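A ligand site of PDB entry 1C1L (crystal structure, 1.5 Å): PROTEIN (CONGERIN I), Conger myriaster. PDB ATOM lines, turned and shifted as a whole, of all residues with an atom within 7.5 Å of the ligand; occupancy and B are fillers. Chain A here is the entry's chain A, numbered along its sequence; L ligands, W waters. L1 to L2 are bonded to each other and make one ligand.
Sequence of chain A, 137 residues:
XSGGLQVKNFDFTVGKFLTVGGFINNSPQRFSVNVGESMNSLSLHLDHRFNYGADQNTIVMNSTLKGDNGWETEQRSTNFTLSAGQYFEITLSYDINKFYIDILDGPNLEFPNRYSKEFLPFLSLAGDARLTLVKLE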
ATOM      1  N   ARG A  30     -22.241  -3.512  -2.295  1.00  0.00           N
ATOM      2  CA  ARG A  30     -22.083  -2.257  -1.585  1.00  0.00           C
ATOM      3  C   ARG A  30     -20.829  -1.548  -2.047  1.00  0.00           C
ATOM      4  O   ARG A  30     -19.976  -2.193  -2.668  1.00  0.00           O
ATOM      5  CB  ARG A  30     -21.942  -2.497  -0.072  1.00  0.00           C
ATOM      6  CG  ARG A  30     -20.736  -3.368   0.306  1.00  0.00           C
ATOM      7  CD  ARG A  30     -20.827  -3.606   1.799  1.00  0.00           C
ATOM      8  NE  ARG A  30     -19.763  -4.464   2.284  1.00  0.00           N
ATOM      9  CZ  ARG A  30     -19.011  -4.167   3.342  1.00  0.00           C
ATOM     10  NH1 ARG A  30     -19.163  -3.044   4.050  1.00  0.00           N
ATOM     11  NH2 ARG A  30     -18.064  -5.021   3.707  1.00  0.00           N
ATOM     12  N   SER A  32     -18.110   1.924  -0.615  1.00  0.00           N
ATOM     13  CA  SER A  32     -17.900   3.005   0.321  1.00  0.00           C
ATOM     14  C   SER A  32     -16.930   4.071  -0.158  1.00  0.00           C
ATOM     15  O   SER A  32     -16.037   3.844  -0.971  1.00  0.00           O
ATOM     16  CB  SER A  32     -17.383   2.445   1.627  1.00  0.00           C
ATOM     17  OG  SER A  32     -16.246   1.608   1.437  1.00  0.00           O
ATOM     18  N   ASN A  34     -14.299   6.515   1.608  1.00  0.00           N
ATOM     19  CA  ASN A  34     -13.509   6.531   2.822  1.00  0.00           C
ATOM     20  C   ASN A  34     -12.569   7.718   2.842  1.00  0.00           C
ATOM     21  O   ASN A  34     -11.791   7.872   1.904  1.00  0.00           O
ATOM     22  CB  ASN A  34     -12.670   5.266   2.918  1.00  0.00           C
ATOM     23  CG  ASN A  34     -13.517   4.031   2.768  1.00  0.00           C
ATOM     24  OD1 ASN A  34     -14.160   3.563   3.718  1.00  0.00           O
ATOM     25  ND2 ASN A  34     -13.630   3.487   1.555  1.00  0.00           N
ATOM     26  N   HIS A  45     -16.382   6.578   6.916  1.00  0.00           N
ATOM     27  CA  HIS A  45     -16.582   5.442   6.044  1.00  0.00           C
ATOM     28  C   HIS A  45     -18.047   5.584   5.700  1.00  0.00           C
ATOM     29  O   HIS A  45     -18.881   5.488   6.602  1.00  0.00           O
ATOM     30  CB  HIS A  45     -16.335   4.138   6.784  1.00  0.00           C
ATOM     31  CG  HIS A  45     -16.787   2.863   6.074  1.00  0.00           C
ATOM     32  ND1 HIS A  45     -16.234   2.231   5.060  1.00  0.00           N
ATOM     33  CD2 HIS A  45     -17.859   2.108   6.478  1.00  0.00           C
ATOM     34  CE1 HIS A  45     -16.913   1.135   4.826  1.00  0.00           C
ATOM     35  NE2 HIS A  45     -17.892   1.079   5.681  1.00  0.00           N
ATOM     36  N   LEU A  46     -18.410   5.828   4.447  1.00  0.00           N
ATOM     37  CA  LEU A  46     -19.785   6.034   4.033  1.00  0.00           C
ATOM     38  C   LEU A  46     -20.117   4.881   3.119  1.00  0.00           C
ATOM     39  O   LEU A  46     -19.678   4.840   1.962  1.00  0.00           O
ATOM     40  CB  LEU A  46     -19.895   7.372   3.301  1.00  0.00           C
ATOM     41  CG  LEU A  46     -21.227   7.681   2.602  1.00  0.00           C
ATOM     42  CD1 LEU A  46     -22.324   7.883   3.620  1.00  0.00           C
ATOM     43  CD2 LEU A  46     -21.065   8.899   1.728  1.00  0.00           C
ATOM     44  N   ASP A  47     -20.880   3.915   3.633  1.00  0.00           N
ATOM     45  CA  ASP A  47     -21.167   2.682   2.916  1.00  0.00           C
ATOM     46  C   ASP A  47     -22.603   2.630   2.384  1.00  0.00           C
ATOM     47  O   ASP A  47     -23.560   2.770   3.150  1.00  0.00           O
ATOM     48  CB  ASP A  47     -20.889   1.520   3.876  1.00  0.00           C
ATOM     49  CG  ASP A  47     -20.601   0.190   3.214  1.00  0.00           C
ATOM     50  OD1 ASP A  47     -20.157   0.123   2.072  1.00  0.00           O
ATOM     51  OD2 ASP A  47     -20.816  -0.817   3.866  1.00  0.00           O
ATOM     52  N   ARG A  49     -25.121   0.260   0.973  1.00  0.00           N
ATOM     53  CA  ARG A  49     -25.348  -1.166   0.876  1.00  0.00           C
ATOM     54  C   ARG A  49     -26.638  -1.425   0.118  1.00  0.00           C
ATOM     55  O   ARG A  49     -27.742  -1.079   0.559  1.00  0.00           O
ATOM     56  CB  ARG A  49     -25.443  -1.777   2.277  1.00  0.00           C
ATOM     57  CG  ARG A  49     -24.196  -1.535   3.102  1.00  0.00           C
ATOM     58  CD  ARG A  49     -24.346  -2.127   4.480  1.00  0.00           C
ATOM     59  NE  ARG A  49     -23.068  -2.031   5.139  1.00  0.00           N
ATOM     60  CZ  ARG A  49     -22.758  -2.489   6.338  1.00  0.00           C
ATOM     61  NH1 ARG A  49     -23.669  -3.094   7.090  1.00  0.00           N
ATOM     62  NH2 ARG A  49     -21.520  -2.329   6.805  1.00  0.00           N
ATOM     63  N   TYR A  52     -26.969  -6.553   0.660  1.00  0.00           N
ATOM     64  CA  TYR A  52     -25.944  -7.025   1.545  1.00  0.00           C
ATOM     65  C   TYR A  52     -26.613  -7.711   2.715  1.00  0.00           C
ATOM     66  O   TYR A  52     -26.699  -7.195   3.831  1.00  0.00           O
ATOM     67  CB  TYR A  52     -25.109  -5.810   1.960  1.00  0.00           C
ATOM     68  CG  TYR A  52     -23.902  -6.180   2.793  1.00  0.00           C
ATOM     69  CD1 TYR A  52     -22.869  -6.910   2.205  1.00  0.00           C
ATOM     70  CD2 TYR A  52     -23.806  -5.771   4.119  1.00  0.00           C
ATOM     71  CE1 TYR A  52     -21.740  -7.231   2.941  1.00  0.00           C
ATOM     72  CE2 TYR A  52     -22.684  -6.100   4.878  1.00  0.00           C
ATOM     73  CZ  TYR A  52     -21.659  -6.825   4.266  1.00  0.00           C
ATOM     74  OH  TYR A  52     -20.508  -7.112   4.972  1.00  0.00           O
ATOM     75  N   ASP A  55     -29.036  -6.044   5.216  1.00  0.00           N
ATOM     76  CA  ASP A  55     -29.016  -4.659   4.784  1.00  0.00           C
ATOM     77  C   ASP A  55     -29.328  -4.568   3.319  1.00  0.00           C
ATOM     78  O   ASP A  55     -28.593  -5.054   2.450  1.00  0.00           O
ATOM     79  CB  ASP A  55     -27.643  -4.078   5.057  1.00  0.00           C
ATOM     80  CG  ASP A  55     -27.412  -3.873   6.533  1.00  0.00           C
ATOM     81  OD1 ASP A  55     -28.371  -3.596   7.268  1.00  0.00           O
ATOM     82  OD2 ASP A  55     -26.277  -3.997   6.960  1.00  0.00           O
ATOM     83  N   VAL A  60     -24.704   3.125   5.763  1.00  0.00           N
ATOM     84  CA  VAL A  60     -24.060   2.916   7.042  1.00  0.00           C
ATOM     85  C   VAL A  60     -22.864   3.856   7.085  1.00  0.00           C
ATOM     86  O   VAL A  60     -22.034   3.851   6.172  1.00  0.00           O
ATOM     87  CB  VAL A  60     -23.578   1.458   7.186  1.00  0.00           C
ATOM     88  CG1 VAL A  60     -22.813   1.285   8.496  1.00  0.00           C
ATOM     89  CG2 VAL A  60     -24.773   0.507   7.171  1.00  0.00           C
ATOM     90  N   MET A  61     -22.755   4.634   8.143  1.00  0.00           N
ATOM     91  CA  MET A  61     -21.642   5.540   8.366  1.00  0.00           C
ATOM     92  C   MET A  61     -20.941   5.130   9.642  1.00  0.00           C
ATOM     93  O   MET A  61     -21.573   4.778  10.651  1.00  0.00           O
ATOM     94  CB  MET A  61     -22.148   6.963   8.513  1.00  0.00           C
ATOM     95  CG  MET A  61     -22.758   7.481   7.222  1.00  0.00           C
ATOM     96  SD  MET A  61     -23.447   9.126   7.445  1.00  0.00           S
ATOM     97  CE  MET A  61     -25.059   8.653   8.030  1.00  0.00           C
ATOM     98  N   ASN A  62     -19.613   5.169   9.599  1.00  0.00           N
ATOM     99  CA  ASN A  62     -18.831   4.816  10.762  1.00  0.00           C
ATOM    100  C   ASN A  62     -17.428   5.382  10.586  1.00  0.00           C
ATOM    101  O   ASN A  62     -17.149   6.042   9.575  1.00  0.00           O
ATOM    102  CB  ASN A  62     -18.784   3.293  10.879  1.00  0.00           C
ATOM    103  CG  ASN A  62     -18.602   2.821  12.310  1.00  0.00           C
ATOM    104  OD1 ASN A  62     -18.255   3.585  13.218  1.00  0.00           O
ATOM    105  ND2 ASN A  62     -18.792   1.543  12.567  1.00  0.00           N
ATOM    106  N   SER A  63     -16.555   5.122  11.553  1.00  0.00           N
ATOM    107  CA  SER A  63     -15.161   5.478  11.547  1.00  0.00           C
ATOM    108  C   SER A  63     -14.393   4.329  12.211  1.00  0.00           C
ATOM    109  O   SER A  63     -14.986   3.396  12.776  1.00  0.00           O
ATOM    110  CB  SER A  63     -14.988   6.771  12.342  1.00  0.00           C
ATOM    111  OG  SER A  63     -15.332   6.613  13.708  1.00  0.00           O
ATOM    112  N   ASP A  68     -10.237  -2.734  10.017  1.00  0.00           N
ATOM    113  CA  ASP A  68     -11.404  -3.590  10.134  1.00  0.00           C
ATOM    114  C   ASP A  68     -11.679  -4.071  11.560  1.00  0.00           C
ATOM    115  O   ASP A  68     -12.758  -4.586  11.834  1.00  0.00           O
ATOM    116  CB  ASP A  68     -11.223  -4.776   9.200  1.00  0.00           C
ATOM    117  CG  ASP A  68     -12.524  -5.494   8.903  1.00  0.00           C
ATOM    118  OD1 ASP A  68     -13.541  -4.854   8.646  1.00  0.00           O
ATOM    119  OD2 ASP A  68     -12.535  -6.731   8.944  1.00  0.00           O
ATOM    120  N   ASN A  69     -10.740  -3.907  12.476  1.00  0.00           N
ATOM    121  CA  ASN A  69     -11.015  -4.315  13.852  1.00  0.00           C
ATOM    122  C   ASN A  69     -11.343  -3.151  14.762  1.00  0.00           C
ATOM    123  O   ASN A  69     -11.352  -3.299  15.983  1.00  0.00           O
ATOM    124  CB  ASN A  69      -9.831  -5.111  14.400  1.00  0.00           C
ATOM    125  CG  ASN A  69      -9.821  -6.462  13.715  1.00  0.00           C
ATOM    126  OD1 ASN A  69     -10.786  -7.220  13.699  1.00  0.00           O
ATOM    127  ND2 ASN A  69      -8.768  -6.767  12.981  1.00  0.00           N
ATOM    128  N   GLY A  70     -11.619  -1.959  14.229  1.00  0.00           N
ATOM    129  CA  GLY A  70     -11.904  -0.840  15.112  1.00  0.00           C
ATOM    130  C   GLY A  70     -13.194  -0.143  14.776  1.00  0.00           C
ATOM    131  O   GLY A  70     -13.348   0.999  15.202  1.00  0.00           O
ATOM    132  N   TRP A  71     -14.108  -0.707  13.993  1.00  0.00           N
ATOM    133  CA  TRP A  71     -15.354  -0.034  13.638  1.00  0.00           C
ATOM    134  C   TRP A  71     -16.112   0.332  14.895  1.00  0.00           C
ATOM    135  O   TRP A  71     -16.231  -0.503  15.800  1.00  0.00           O
ATOM    136  CB  TRP A  71     -16.222  -0.911  12.759  1.00  0.00           C
ATOM    137  CG  TRP A  71     -15.585  -1.240  11.421  1.00  0.00           C
ATOM    138  CD1 TRP A  71     -15.242  -2.521  11.092  1.00  0.00           C
ATOM    139  CD2 TRP A  71     -15.286  -0.344  10.429  1.00  0.00           C
ATOM    140  NE1 TRP A  71     -14.736  -2.444   9.886  1.00  0.00           N
ATOM    141  CE2 TRP A  71     -14.752  -1.173   9.447  1.00  0.00           C
ATOM    142  CE3 TRP A  71     -15.422   1.030  10.218  1.00  0.00           C
ATOM    143  CZ2 TRP A  71     -14.311  -0.617   8.238  1.00  0.00           C
ATOM    144  CZ3 TRP A  71     -14.987   1.580   9.014  1.00  0.00           C
ATOM    145  CH2 TRP A  71     -14.441   0.763   8.021  1.00  0.00           C
ATOM    146  N   GLU A  72     -16.600   1.562  14.940  1.00  0.00           N
ATOM    147  CA  GLU A  72     -17.234   2.062  16.134  1.00  0.00           C
ATOM    148  C   GLU A  72     -18.760   2.070  16.012  1.00  0.00           C
ATOM    149  O   GLU A  72     -19.322   1.155  15.401  1.00  0.00           O
ATOM    150  CB  GLU A  72     -16.658   3.451  16.390  1.00  0.00           C
ATOM    151  CG  GLU A  72     -15.141   3.471  16.555  1.00  0.00           C
ATOM    152  CD  GLU A  72     -14.566   4.769  17.081  1.00  0.00           C
ATOM    153  OE1 GLU A  72     -15.309   5.578  17.618  1.00  0.00           O
ATOM    154  OE2 GLU A  72     -13.359   4.963  16.963  1.00  0.00           O
ATOM    155  N   THR A  73     -19.480   3.045  16.586  1.00  0.00           N
ATOM    156  CA  THR A  73     -20.926   3.112  16.456  1.00  0.00           C
ATOM    157  C   THR A  73     -21.400   3.515  15.065  1.00  0.00           C
ATOM    158  O   THR A  73     -21.079   4.565  14.538  1.00  0.00           O
ATOM    159  CB  THR A  73     -21.464   4.121  17.498  1.00  0.00           C
ATOM    160  OG1 THR A  73     -20.996   3.654  18.760  1.00  0.00           O
ATOM    161  CG2 THR A  73     -22.999   4.250  17.500  1.00  0.00           C
ATOM    162  N   GLU A  74     -22.156   2.620  14.443  1.00  0.00           N
ATOM    163  CA  GLU A  74     -22.762   2.915  13.158  1.00  0.00           C
ATOM    164  C   GLU A  74     -23.915   3.887  13.298  1.00  0.00           C
ATOM    165  O   GLU A  74     -24.640   3.919  14.293  1.00  0.00           O
ATOM    166  CB  GLU A  74     -23.333   1.657  12.527  1.00  0.00           C
ATOM    167  CG  GLU A  74     -22.255   0.631  12.268  1.00  0.00           C
ATOM    168  CD  GLU A  74     -22.751  -0.617  11.559  1.00  0.00           C
ATOM    169  OE1 GLU A  74     -23.935  -0.909  11.580  1.00  0.00           O
ATOM    170  OE2 GLU A  74     -21.926  -1.303  10.974  1.00  0.00           O
ATOM    171  N   GLN A  75     -24.008   4.778  12.304  1.00  0.00           N
ATOM    172  CA  GLN A  75     -25.175   5.595  12.107  1.00  0.00           C
ATOM    173  C   GLN A  75     -25.673   5.143  10.740  1.00  0.00           C
ATOM    174  O   GLN A  75     -24.934   4.954   9.787  1.00  0.00           O
ATOM    175  CB  GLN A  75     -24.818   7.076  12.110  1.00  0.00           C
ATOM    176  CG  GLN A  75     -24.397   7.479  13.522  1.00  0.00           C
ATOM    177  CD  GLN A  75     -24.469   8.980  13.773  1.00  0.00           C
ATOM    178  OE1 GLN A  75     -25.130   9.686  13.024  1.00  0.00           O
ATOM    179  NE2 GLN A  75     -23.881   9.501  14.832  1.00  0.00           N
ATOM    180  N   ARG A  76     -26.962   4.824  10.678  1.00  0.00           N
ATOM    181  CA  ARG A  76     -27.616   4.275   9.504  1.00  0.00           C
ATOM    182  C   ARG A  76     -28.697   5.178   8.995  1.00  0.00           C
ATOM    183  O   ARG A  76     -29.299   5.949   9.759  1.00  0.00           O
ATOM    184  CB  ARG A  76     -28.237   2.929   9.815  1.00  0.00           C
ATOM    185  CG  ARG A  76     -27.170   1.902  10.090  1.00  0.00           C
ATOM    186  CD  ARG A  76     -27.734   0.638  10.696  1.00  0.00           C
ATOM    187  NE  ARG A  76     -26.698  -0.369  10.694  1.00  0.00           N
ATOM    188  CZ  ARG A  76     -26.765  -1.398   9.854  1.00  0.00           C
ATOM    189  NH1 ARG A  76     -27.788  -1.511   9.022  1.00  0.00           N
ATOM    190  NH2 ARG A  76     -25.783  -2.296   9.804  1.00  0.00           N
HETATM  191  C1  LIG L   1     -22.885  -4.619  11.740  1.00  0.00           C
HETATM  192  C2  LIG L   1     -22.230  -4.592  10.348  1.00  0.00           C
HETATM  193  C3  LIG L   1     -20.719  -4.576  10.501  1.00  0.00           C
HETATM  194  C4  LIG L   1     -20.279  -5.772  11.353  1.00  0.00           C
HETATM  195  C5  LIG L   1     -18.776  -5.828  11.567  1.00  0.00           C
HETATM  196  C6  LIG L   1     -22.339  -5.769  12.577  1.00  0.00           C
HETATM  197  O1  LIG L   1     -22.823  -5.691  13.847  1.00  0.00           O
HETATM  198  O2  LIG L   1     -24.284  -4.762  11.584  1.00  0.00           O
HETATM  199  O3  LIG L   1     -22.653  -3.440   9.644  1.00  0.00           O
HETATM  200  O4  LIG L   1     -20.098  -4.666   9.183  1.00  0.00           O
HETATM  201  O5  LIG L   1     -20.901  -5.671  12.643  1.00  0.00           O
HETATM  202  O6  LIG L   1     -18.302  -4.656  12.215  1.00  0.00           O
HETATM  203  C1  LG2 L   2     -19.007  -3.856   8.953  1.00  0.00           C
HETATM  204  C2  LG2 L   2     -18.402  -4.165   7.581  1.00  0.00           C
HETATM  205  C3  LG2 L   2     -17.284  -3.173   7.250  1.00  0.00           C
HETATM  206  C4  LG2 L   2     -17.782  -1.725   7.417  1.00  0.00           C
HETATM  207  C5  LG2 L   2     -18.434  -1.551   8.785  1.00  0.00           C
HETATM  208  C6  LG2 L   2     -19.025  -0.174   8.970  1.00  0.00           C
HETATM  209  O1  LG2 L   2     -17.881  -5.486   7.603  1.00  0.00           O
HETATM  210  O2  LG2 L   2     -16.863  -3.397   5.922  1.00  0.00           O
HETATM  211  O3  LG2 L   2     -18.715  -1.440   6.387  1.00  0.00           O
HETATM  212  O4  LG2 L   2     -19.492  -2.514   8.981  1.00  0.00           O
HETATM  213  O5  LG2 L   2     -19.564  -0.023  10.263  1.00  0.00           O
HETATM  214  O   HOH W   1     -20.124  -6.968   7.534  1.00  0.00           O
HETATM  215  O   HOH W   2     -19.552  -1.773  12.464  1.00  0.00           O
HETATM  216  O   HOH W   3     -15.782  -6.348   9.314  1.00  0.00           O
HETATM  217  O   HOH W   4     -15.840  -1.996   3.598  1.00  0.00           O
HETATM  218  O   HOH W   5     -14.301  -4.116   6.171  1.00  0.00           O
HETATM  219  O   HOH W   6     -18.983  -7.127  14.819  1.00  0.00           O
HETATM  220  O   HOH W   7     -17.368  -4.210  14.840  1.00  0.00           O
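OE2 of Glu 74 is in hydrogen-bond range of O3 of LIG L1 (2.6 Å).
NE2 of His 45 lies within hydrogen-bond range of O3 of LG2 L2.
NH1 of Arg 49 is in hydrogen-bond range of O3 of LIG L1 (2.8 Å).
The guanidinium group of Arg 30 sits at hydrogen-bond distance from an oxygen (O3) of LG2 L2, at 2.9 Å.
An oxygen (O5) of LG2 L2 sits at hydrogen-bond distance from the side-chain amide nitrogen of Asn 62 (2.9 Å).
The guanidinium group (NH2) of Arg 76 lies within hydrogen-bond range of an oxygen (O3) of LIG L1 (3.3 Å).
The side-chain carboxylate of Asp 47 sits at hydrogen-bond distance from an oxygen (O3) of LG2 L2, 3.3 Å away.
The guanidinium group of Arg 76 is in salt-bridge range of the side-chain carboxylate of Glu 74 (2.9 Å).
The backbone NH of His 45 is in hydrogen-bond range of the backbone carbonyl oxygen of Asn 62.
NE of Arg 49 lies within salt-bridge range of OD2 of Asp 47.
The guanidinium group (NH1) of Arg 49 lies within salt-bridge range of the side-chain carboxylate (OD2) of Asp 55 (2.8 Å).
The guanidinium group (NH1) of Arg 30 lies within salt-bridge range of the side-chain carboxylate (OD2) of Asp 47 (2.8 Å).
The side-chain amide nitrogen (ND2) of Asn 62 is in hydrogen-bond range of the backbone carbonyl oxygen (O) of Glu 72 (2.9 Å).
O of Thr 73 lies close to OD1 of Asn 62 (3.3 Å).
The indole nitrogen (NE1) of Trp 71 is in hydrogen-bond range of the side-chain carboxylate (OD1) of Asp 68 (3.0 Å).
Residues that only touch the ligand: Val 60 (3.9 Å) and Trp 71 (3.7 Å).
Hydrophobic or aromatic side chains within 4 Å of the ligand: His 45, Val 60 and Trp 71.
Within 4 Å of the ligand: Arg 30, His 45, Asp 47, Arg 49, Val 60, Asn 62, Trp 71, Glu 74 and Arg 76.
The nearest printed residue that does not touch the ligand is Tyr 52 (4.1 Å).
Water W5 lies within hydrogen-bond range of an oxygen (O2) of LG2 L2 and the side-chain carboxylate of Asp 68.
Water W1 lies within hydrogen-bond range of OH of Tyr 52 (2.6 Å) and O1 of LG2 L2 (2.7 Å).
Water W2 lies within hydrogen-bond range of O5 of LG2 L2 (2.8 Å), OE2 of Glu 74 (2.8 Å) and ND2 of Asn 62 (3.4 Å).
Water W3 bridges the side-chain carboxylate (OD1) of Asp 68 (2.8 Å) and an oxygen (O1) of LG2 L2 (2.8 Å).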
